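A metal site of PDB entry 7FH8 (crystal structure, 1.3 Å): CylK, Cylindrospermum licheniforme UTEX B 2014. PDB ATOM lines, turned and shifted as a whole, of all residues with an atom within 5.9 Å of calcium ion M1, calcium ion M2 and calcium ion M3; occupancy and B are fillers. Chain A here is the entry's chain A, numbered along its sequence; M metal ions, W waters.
Water W1 bridges OD2 of Asp 188 and OD2 of Asp 182.
Within 4 Å of calcium ion M3: Asp 132, Trp 151, Asp 153, Glu 187 and Asp 188.
Within 4 Å of calcium ion M2: Thr 84, Ser 86, Asp 88, Gly 104, Arg 105, His 106 and Asp 109.
The backbone carbonyl oxygen (O) of Leu 83 is in hydrogen-bond range of the guanidinium group (NH1) of Arg 105, at 2.9 Å. The backbone NH of Asp 132 is in hydrogen-bond range of the side-chain carboxylate of Asp 182. NE1 of Trp 103 is in hydrogen-bond range of O of Asp 132, 3.0 Å away. The side-chain carboxylate of Glu 187 is in hydrogen-bond range of the side-chain hydroxyl of Ser 150. OG of Ser 86 is in hydrogen-bond range of OG1 of Thr 84, 2.8 Å away. The backbone NH (N) of Gly 104 lies within hydrogen-bond range of the backbone carbonyl oxygen (O) of Leu 130. OD1 of Asp 182 sits at hydrogen-bond distance from N of Gly 131 (2.8 Å). O of Glu 187 sits at hydrogen-bond distance from OG of Ser 152, 2.9 Å away.
Calcium ion M1 is bound by OD2 of Asp 109, OD1 of Asp 132, O of Gly 131, OD1 of Asp 153, O of Gly 107 and O of Arg 105.
Calcium ion M2 is bound by O of Ser 86, O of His 106, O of Gly 104, O of Thr 84, OD2 of Asp 88 and OD1 of Asp 109. Calcium ion M2 has six donor atoms within binding distance. Slightly farther from calcium ion M2 lies the side-chain carboxylate (OD2) of Asp 109 (3.1 Å).
O of Trp 151 is bound to calcium ion M3. Calcium ion M3 is bound by the side-chain carboxylate (OD2) of Asp 153 (2.3 Å). Water W1 binds calcium ion M3. OD2 of Asp 132 is bound to calcium ion M3 (2.4 Å). OE2 of Glu 187 is bound to calcium ion M3 (2.4 Å). OD1 of Asp 188 binds calcium ion M3 (2.4 Å).
Of the 26 residues printed, 7 come within 4 Å of calcium ion M1.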
ATOM      1  N   LEU A  83     -24.489  21.143  -7.962  1.00  0.00           N
ATOM      2  CA  LEU A  83     -23.676  22.324  -8.188  1.00  0.00           C
ATOM      3  C   LEU A  83     -23.409  22.498  -9.686  1.00  0.00           C
ATOM      4  O   LEU A  83     -24.086  21.889 -10.520  1.00  0.00           O
ATOM      5  CB  LEU A  83     -22.446  22.295  -7.274  1.00  0.00           C
ATOM      6  CG  LEU A  83     -22.847  22.373  -5.806  1.00  0.00           C
ATOM      7  CD1 LEU A  83     -21.665  22.090  -4.920  1.00  0.00           C
ATOM      8  CD2 LEU A  83     -23.412  23.747  -5.491  1.00  0.00           C
ATOM      9  N   THR A  84     -22.444  23.341 -10.059  1.00  0.00           N
ATOM     10  CA  THR A  84     -22.297  23.777 -11.448  1.00  0.00           C
ATOM     11  C   THR A  84     -21.057  23.166 -12.086  1.00  0.00           C
ATOM     12  O   THR A  84     -20.293  22.428 -11.454  1.00  0.00           O
ATOM     13  CB  THR A  84     -22.261  25.311 -11.576  1.00  0.00           C
ATOM     14  OG1 THR A  84     -20.943  25.818 -11.287  1.00  0.00           O
ATOM     15  CG2 THR A  84     -23.296  25.983 -10.667  1.00  0.00           C
ATOM     16  N   VAL A  85     -20.846  23.509 -13.358  1.00  0.00           N
ATOM     17  CA  VAL A  85     -19.626  23.111 -14.057  1.00  0.00           C
ATOM     18  C   VAL A  85     -18.411  23.897 -13.573  1.00  0.00           C
ATOM     19  O   VAL A  85     -17.283  23.556 -13.922  1.00  0.00           O
ATOM     20  CB  VAL A  85     -19.889  23.175 -15.578  1.00  0.00           C
ATOM     21  CG1 VAL A  85     -18.706  22.650 -16.373  1.00  0.00           C
ATOM     22  CG2 VAL A  85     -21.144  22.397 -15.947  1.00  0.00           C
ATOM     23  N   SER A  86     -18.624  24.937 -12.769  1.00  0.00           N
ATOM     24  CA  SER A  86     -17.567  25.763 -12.206  1.00  0.00           C
ATOM     25  C   SER A  86     -16.920  25.074 -11.017  1.00  0.00           C
ATOM     26  O   SER A  86     -17.417  24.073 -10.491  1.00  0.00           O
ATOM     27  CB  SER A  86     -18.139  27.080 -11.670  1.00  0.00           C
ATOM     28  OG  SER A  86     -19.153  27.588 -12.523  1.00  0.00           O
ATOM     29  N   SER A  87     -15.807  25.650 -10.546  1.00  0.00           N
ATOM     30  CA  SER A  87     -15.230  25.251  -9.266  1.00  0.00           C
ATOM     31  C   SER A  87     -16.032  25.941  -8.166  1.00  0.00           C
ATOM     32  O   SER A  87     -15.878  27.137  -7.920  1.00  0.00           O
ATOM     33  CB  SER A  87     -13.758  25.638  -9.208  1.00  0.00           C
ATOM     34  OG  SER A  87     -13.058  24.942 -10.222  1.00  0.00           O
ATOM     35  N   ASP A  88     -16.925  25.176  -7.522  1.00  0.00           N
ATOM     36  CA  ASP A  88     -17.971  25.750  -6.673  1.00  0.00           C
ATOM     37  C   ASP A  88     -17.651  25.594  -5.193  1.00  0.00           C
ATOM     38  O   ASP A  88     -17.322  24.495  -4.736  1.00  0.00           O
ATOM     39  CB  ASP A  88     -19.291  24.984  -6.872  1.00  0.00           C
ATOM     40  CG  ASP A  88     -19.792  24.998  -8.294  1.00  0.00           C
ATOM     41  OD1 ASP A  88     -20.083  26.105  -8.810  1.00  0.00           O
ATOM     42  OD2 ASP A  88     -19.933  23.909  -8.884  1.00  0.00           O
ATOM     43  N   TRP A 103     -23.485  17.196  -5.102  1.00  0.00           N
ATOM     44  CA  TRP A 103     -22.891  16.759  -6.361  1.00  0.00           C
ATOM     45  C   TRP A 103     -22.098  17.925  -6.960  1.00  0.00           C
ATOM     46  O   TRP A 103     -22.667  18.885  -7.471  1.00  0.00           O
ATOM     47  CB  TRP A 103     -23.990  16.279  -7.299  1.00  0.00           C
ATOM     48  CG  TRP A 103     -23.524  15.711  -8.596  1.00  0.00           C
ATOM     49  CD1 TRP A 103     -22.280  15.226  -8.889  1.00  0.00           C
ATOM     50  CD2 TRP A 103     -24.292  15.573  -9.789  1.00  0.00           C
ATOM     51  NE1 TRP A 103     -22.235  14.780 -10.192  1.00  0.00           N
ATOM     52  CE2 TRP A 103     -23.465  14.976 -10.758  1.00  0.00           C
ATOM     53  CE3 TRP A 103     -25.618  15.894 -10.131  1.00  0.00           C
ATOM     54  CZ2 TRP A 103     -23.906  14.715 -12.053  1.00  0.00           C
ATOM     55  CZ3 TRP A 103     -26.041  15.634 -11.418  1.00  0.00           C
ATOM     56  CH2 TRP A 103     -25.191  15.048 -12.365  1.00  0.00           C
ATOM     57  N   GLY A 104     -20.758  17.817  -6.906  1.00  0.00           N
ATOM     58  CA  GLY A 104     -19.921  18.926  -7.349  1.00  0.00           C
ATOM     59  C   GLY A 104     -19.849  19.101  -8.854  1.00  0.00           C
ATOM     60  O   GLY A 104     -19.704  20.228  -9.343  1.00  0.00           O
ATOM     61  N   ARG A 105     -19.939  18.009  -9.608  1.00  0.00           N
ATOM     62  CA  ARG A 105     -19.747  18.041 -11.066  1.00  0.00           C
ATOM     63  C   ARG A 105     -18.353  18.570 -11.399  1.00  0.00           C
ATOM     64  O   ARG A 105     -17.415  18.431 -10.602  1.00  0.00           O
ATOM     65  CB  ARG A 105     -20.918  18.706 -11.784  1.00  0.00           C
ATOM     66  CG  ARG A 105     -22.218  17.935 -11.603  1.00  0.00           C
ATOM     67  CD  ARG A 105     -23.430  18.719 -12.073  1.00  0.00           C
ATOM     68  NE  ARG A 105     -23.460  18.970 -13.504  1.00  0.00           N
ATOM     69  CZ  ARG A 105     -23.820  20.114 -14.068  1.00  0.00           C
ATOM     70  NH1 ARG A 105     -24.146  21.169 -13.334  1.00  0.00           N
ATOM     71  NH2 ARG A 105     -23.883  20.194 -15.402  1.00  0.00           N
ATOM     72  N   HIS A 106     -18.190  19.174 -12.575  1.00  0.00           N
ATOM     73  CA  HIS A 106     -16.875  19.592 -13.009  1.00  0.00           C
ATOM     74  C   HIS A 106     -16.331  20.676 -12.092  1.00  0.00           C
ATOM     75  O   HIS A 106     -17.059  21.317 -11.327  1.00  0.00           O
ATOM     76  CB  HIS A 106     -16.932  20.162 -14.427  1.00  0.00           C
ATOM     77  CG  HIS A 106     -17.794  19.371 -15.362  1.00  0.00           C
ATOM     78  ND1 HIS A 106     -19.163  19.279 -15.199  1.00  0.00           N
ATOM     79  CD2 HIS A 106     -17.499  18.663 -16.475  1.00  0.00           C
ATOM     80  CE1 HIS A 106     -19.662  18.536 -16.169  1.00  0.00           C
ATOM     81  NE2 HIS A 106     -18.677  18.153 -16.957  1.00  0.00           N
ATOM     82  N   GLY A 107     -15.021  20.898 -12.189  1.00  0.00           N
ATOM     83  CA  GLY A 107     -14.373  21.920 -11.397  1.00  0.00           C
ATOM     84  C   GLY A 107     -13.867  21.399 -10.064  1.00  0.00           C
ATOM     85  O   GLY A 107     -14.210  20.316  -9.601  1.00  0.00           O
ATOM     86  N   SER A 108     -13.013  22.221  -9.436  1.00  0.00           N
ATOM     87  CA  SER A 108     -12.385  21.897  -8.159  1.00  0.00           C
ATOM     88  C   SER A 108     -13.298  22.436  -7.058  1.00  0.00           C
ATOM     89  O   SER A 108     -13.224  23.604  -6.675  1.00  0.00           O
ATOM     90  CB  SER A 108     -11.015  22.556  -8.082  1.00  0.00           C
ATOM     91  OG  SER A 108     -10.203  22.137  -9.168  1.00  0.00           O
ATOM     92  N   ASP A 109     -14.186  21.591  -6.564  1.00  0.00           N
ATOM     93  CA  ASP A 109     -15.256  22.051  -5.694  1.00  0.00           C
ATOM     94  C   ASP A 109     -14.860  21.993  -4.224  1.00  0.00           C
ATOM     95  O   ASP A 109     -14.118  21.107  -3.794  1.00  0.00           O
ATOM     96  CB  ASP A 109     -16.526  21.231  -5.921  1.00  0.00           C
ATOM     97  CG  ASP A 109     -16.969  21.274  -7.380  1.00  0.00           C
ATOM     98  OD1 ASP A 109     -17.300  22.384  -7.858  1.00  0.00           O
ATOM     99  OD2 ASP A 109     -16.953  20.226  -8.061  1.00  0.00           O
ATOM    100  N   LEU A 130     -20.466  13.605  -3.957  1.00  0.00           N
ATOM    101  CA  LEU A 130     -19.830  13.243  -5.223  1.00  0.00           C
ATOM    102  C   LEU A 130     -18.988  14.441  -5.642  1.00  0.00           C
ATOM    103  O   LEU A 130     -19.519  15.486  -6.029  1.00  0.00           O
ATOM    104  CB  LEU A 130     -20.884  12.917  -6.287  1.00  0.00           C
ATOM    105  CG  LEU A 130     -21.733  11.669  -6.018  1.00  0.00           C
ATOM    106  CD1 LEU A 130     -23.048  11.769  -6.775  1.00  0.00           C
ATOM    107  CD2 LEU A 130     -20.966  10.434  -6.461  1.00  0.00           C
ATOM    108  N   GLY A 131     -17.660  14.299  -5.554  1.00  0.00           N
ATOM    109  CA  GLY A 131     -16.793  15.423  -5.894  1.00  0.00           C
ATOM    110  C   GLY A 131     -16.874  15.802  -7.355  1.00  0.00           C
ATOM    111  O   GLY A 131     -16.935  16.980  -7.708  1.00  0.00           O
ATOM    112  N   ASP A 132     -16.847  14.791  -8.236  1.00  0.00           N
ATOM    113  CA  ASP A 132     -16.943  15.015  -9.666  1.00  0.00           C
ATOM    114  C   ASP A 132     -18.166  14.293 -10.212  1.00  0.00           C
ATOM    115  O   ASP A 132     -19.248  14.888 -10.253  1.00  0.00           O
ATOM    116  CB  ASP A 132     -15.643  14.585 -10.367  1.00  0.00           C
ATOM    117  CG  ASP A 132     -14.499  15.562 -10.121  1.00  0.00           C
ATOM    118  OD1 ASP A 132     -14.731  16.793 -10.170  1.00  0.00           O
ATOM    119  OD2 ASP A 132     -13.358  15.109  -9.864  1.00  0.00           O
ATOM    120  N   ILE A 134     -18.913  13.476 -13.292  1.00  0.00           N
ATOM    121  CA  ILE A 134     -19.325  14.502 -14.243  1.00  0.00           C
ATOM    122  C   ILE A 134     -20.316  13.968 -15.270  1.00  0.00           C
ATOM    123  O   ILE A 134     -20.446  12.763 -15.496  1.00  0.00           O
ATOM    124  CB  ILE A 134     -18.120  15.189 -14.913  1.00  0.00           C
ATOM    125  CG1 ILE A 134     -17.388  14.207 -15.836  1.00  0.00           C
ATOM    126  CG2 ILE A 134     -17.205  15.824 -13.853  1.00  0.00           C
ATOM    127  CD1 ILE A 134     -16.251  14.845 -16.618  1.00  0.00           C
ATOM    128  N   SER A 150     -11.085  14.791 -14.349  1.00  0.00           N
ATOM    129  CA  SER A 150     -11.512  14.963 -12.959  1.00  0.00           C
ATOM    130  C   SER A 150     -10.724  16.113 -12.355  1.00  0.00           C
ATOM    131  O   SER A 150      -9.752  16.600 -12.941  1.00  0.00           O
ATOM    132  CB  SER A 150     -11.346  13.672 -12.156  1.00  0.00           C
ATOM    133  OG  SER A 150     -10.008  13.219 -12.196  1.00  0.00           O
ATOM    134  N   TRP A 151     -11.154  16.540 -11.168  1.00  0.00           N
ATOM    135  CA  TRP A 151     -10.606  17.724 -10.522  1.00  0.00           C
ATOM    136  C   TRP A 151     -10.334  17.414  -9.058  1.00  0.00           C
ATOM    137  O   TRP A 151     -10.890  16.484  -8.484  1.00  0.00           O
ATOM    138  CB  TRP A 151     -11.598  18.894 -10.601  1.00  0.00           C
ATOM    139  CG  TRP A 151     -11.665  19.549 -11.958  1.00  0.00           C
ATOM    140  CD1 TRP A 151     -11.012  20.678 -12.359  1.00  0.00           C
ATOM    141  CD2 TRP A 151     -12.412  19.087 -13.102  1.00  0.00           C
ATOM    142  NE1 TRP A 151     -11.314  20.955 -13.675  1.00  0.00           N
ATOM    143  CE2 TRP A 151     -12.160  19.992 -14.151  1.00  0.00           C
ATOM    144  CE3 TRP A 151     -13.270  18.005 -13.334  1.00  0.00           C
ATOM    145  CZ2 TRP A 151     -12.733  19.847 -15.413  1.00  0.00           C
ATOM    146  CZ3 TRP A 151     -13.823  17.851 -14.589  1.00  0.00           C
ATOM    147  CH2 TRP A 151     -13.559  18.776 -15.619  1.00  0.00           C
ATOM    148  N   SER A 152      -9.476  18.226  -8.440  1.00  0.00           N
ATOM    149  CA  SER A 152      -9.252  18.155  -7.003  1.00  0.00           C
ATOM    150  C   SER A 152     -10.434  18.775  -6.273  1.00  0.00           C
ATOM    151  O   SER A 152     -10.624  19.999  -6.316  1.00  0.00           O
ATOM    152  CB  SER A 152      -7.963  18.897  -6.656  1.00  0.00           C
ATOM    153  OG  SER A 152      -6.836  18.303  -7.264  1.00  0.00           O
ATOM    154  N   ASP A 153     -11.229  17.956  -5.593  1.00  0.00           N
ATOM    155  CA  ASP A 153     -12.321  18.428  -4.775  1.00  0.00           C
ATOM    156  C   ASP A 153     -11.921  18.320  -3.309  1.00  0.00           C
ATOM    157  O   ASP A 153     -11.166  17.418  -2.930  1.00  0.00           O
ATOM    158  CB  ASP A 153     -13.588  17.609  -5.012  1.00  0.00           C
ATOM    159  CG  ASP A 153     -13.964  17.566  -6.462  1.00  0.00           C
ATOM    160  OD1 ASP A 153     -14.355  18.635  -6.994  1.00  0.00           O
ATOM    161  OD2 ASP A 153     -13.861  16.493  -7.087  1.00  0.00           O
ATOM    162  N   PHE A 155     -13.477  17.836   0.388  1.00  0.00           N
ATOM    163  CA  PHE A 155     -14.652  17.371   1.108  1.00  0.00           C
ATOM    164  C   PHE A 155     -14.498  17.835   2.553  1.00  0.00           C
ATOM    165  O   PHE A 155     -13.588  17.388   3.259  1.00  0.00           O
ATOM    166  CB  PHE A 155     -14.789  15.852   1.041  1.00  0.00           C
ATOM    167  CG  PHE A 155     -14.879  15.309  -0.364  1.00  0.00           C
ATOM    168  CD1 PHE A 155     -16.099  15.303  -1.047  1.00  0.00           C
ATOM    169  CD2 PHE A 155     -13.765  14.787  -1.002  1.00  0.00           C
ATOM    170  CE1 PHE A 155     -16.191  14.792  -2.329  1.00  0.00           C
ATOM    171  CE2 PHE A 155     -13.852  14.267  -2.293  1.00  0.00           C
ATOM    172  CZ  PHE A 155     -15.072  14.269  -2.954  1.00  0.00           C
ATOM    173  N   ASP A 182     -16.805   9.056  -4.329  1.00  0.00           N
ATOM    174  CA  ASP A 182     -15.824   9.076  -5.413  1.00  0.00           C
ATOM    175  C   ASP A 182     -14.521   9.722  -4.961  1.00  0.00           C
ATOM    176  O   ASP A 182     -13.854  10.425  -5.732  1.00  0.00           O
ATOM    177  CB  ASP A 182     -16.363   9.788  -6.652  1.00  0.00           C
ATOM    178  CG  ASP A 182     -16.502  11.292  -6.454  1.00  0.00           C
ATOM    179  OD1 ASP A 182     -16.784  11.696  -5.303  1.00  0.00           O
ATOM    180  OD2 ASP A 182     -16.310  12.064  -7.423  1.00  0.00           O
ATOM    181  N   ASN A 184     -10.860  10.285  -4.580  1.00  0.00           N
ATOM    182  CA  ASN A 184      -9.658   9.845  -5.281  1.00  0.00           C
ATOM    183  C   ASN A 184      -8.453  10.399  -4.520  1.00  0.00           C
ATOM    184  O   ASN A 184      -8.202  11.606  -4.592  1.00  0.00           O
ATOM    185  CB  ASN A 184      -9.670  10.360  -6.718  1.00  0.00           C
ATOM    186  CG  ASN A 184      -8.433   9.940  -7.500  1.00  0.00           C
ATOM    187  OD1 ASN A 184      -7.448   9.480  -6.938  1.00  0.00           O
ATOM    188  ND2 ASN A 184      -8.494  10.090  -8.825  1.00  0.00           N
ATOM    189  N   GLU A 187      -5.986  13.036  -6.000  1.00  0.00           N
ATOM    190  CA  GLU A 187      -6.390  14.386  -6.395  1.00  0.00           C
ATOM    191  C   GLU A 187      -7.173  15.108  -5.295  1.00  0.00           C
ATOM    192  O   GLU A 187      -6.976  16.311  -5.095  1.00  0.00           O
ATOM    193  CB  GLU A 187      -7.214  14.360  -7.699  1.00  0.00           C
ATOM    194  CG  GLU A 187      -8.547  13.602  -7.596  1.00  0.00           C
ATOM    195  CD  GLU A 187      -9.421  13.679  -8.854  1.00  0.00           C
ATOM    196  OE1 GLU A 187      -8.856  13.853  -9.959  1.00  0.00           O
ATOM    197  OE2 GLU A 187     -10.668  13.562  -8.740  1.00  0.00           O
ATOM    198  N   ASP A 188      -8.075  14.409  -4.614  1.00  0.00           N
ATOM    199  CA  ASP A 188      -9.017  15.051  -3.712  1.00  0.00           C
ATOM    200  C   ASP A 188      -8.416  15.240  -2.323  1.00  0.00           C
ATOM    201  O   ASP A 188      -7.378  14.650  -1.983  1.00  0.00           O
ATOM    202  CB  ASP A 188     -10.294  14.204  -3.573  1.00  0.00           C
ATOM    203  CG  ASP A 188     -11.072  14.072  -4.868  1.00  0.00           C
ATOM    204  OD1 ASP A 188     -11.123  15.012  -5.683  1.00  0.00           O
ATOM    205  OD2 ASP A 188     -11.669  12.992  -5.074  1.00  0.00           O
HETATM  206 CA    CA M   1     -15.683  18.549  -8.960  1.00  0.00          CA
HETATM  207 CA    CA M   2     -18.596  22.211  -9.832  1.00  0.00          CA
HETATM  208 CA    CA M   3     -12.337  14.904  -7.756  1.00  0.00          CA
HETATM  209  O   HOH W   1     -13.726  13.219  -6.895  1.00  0.00           O
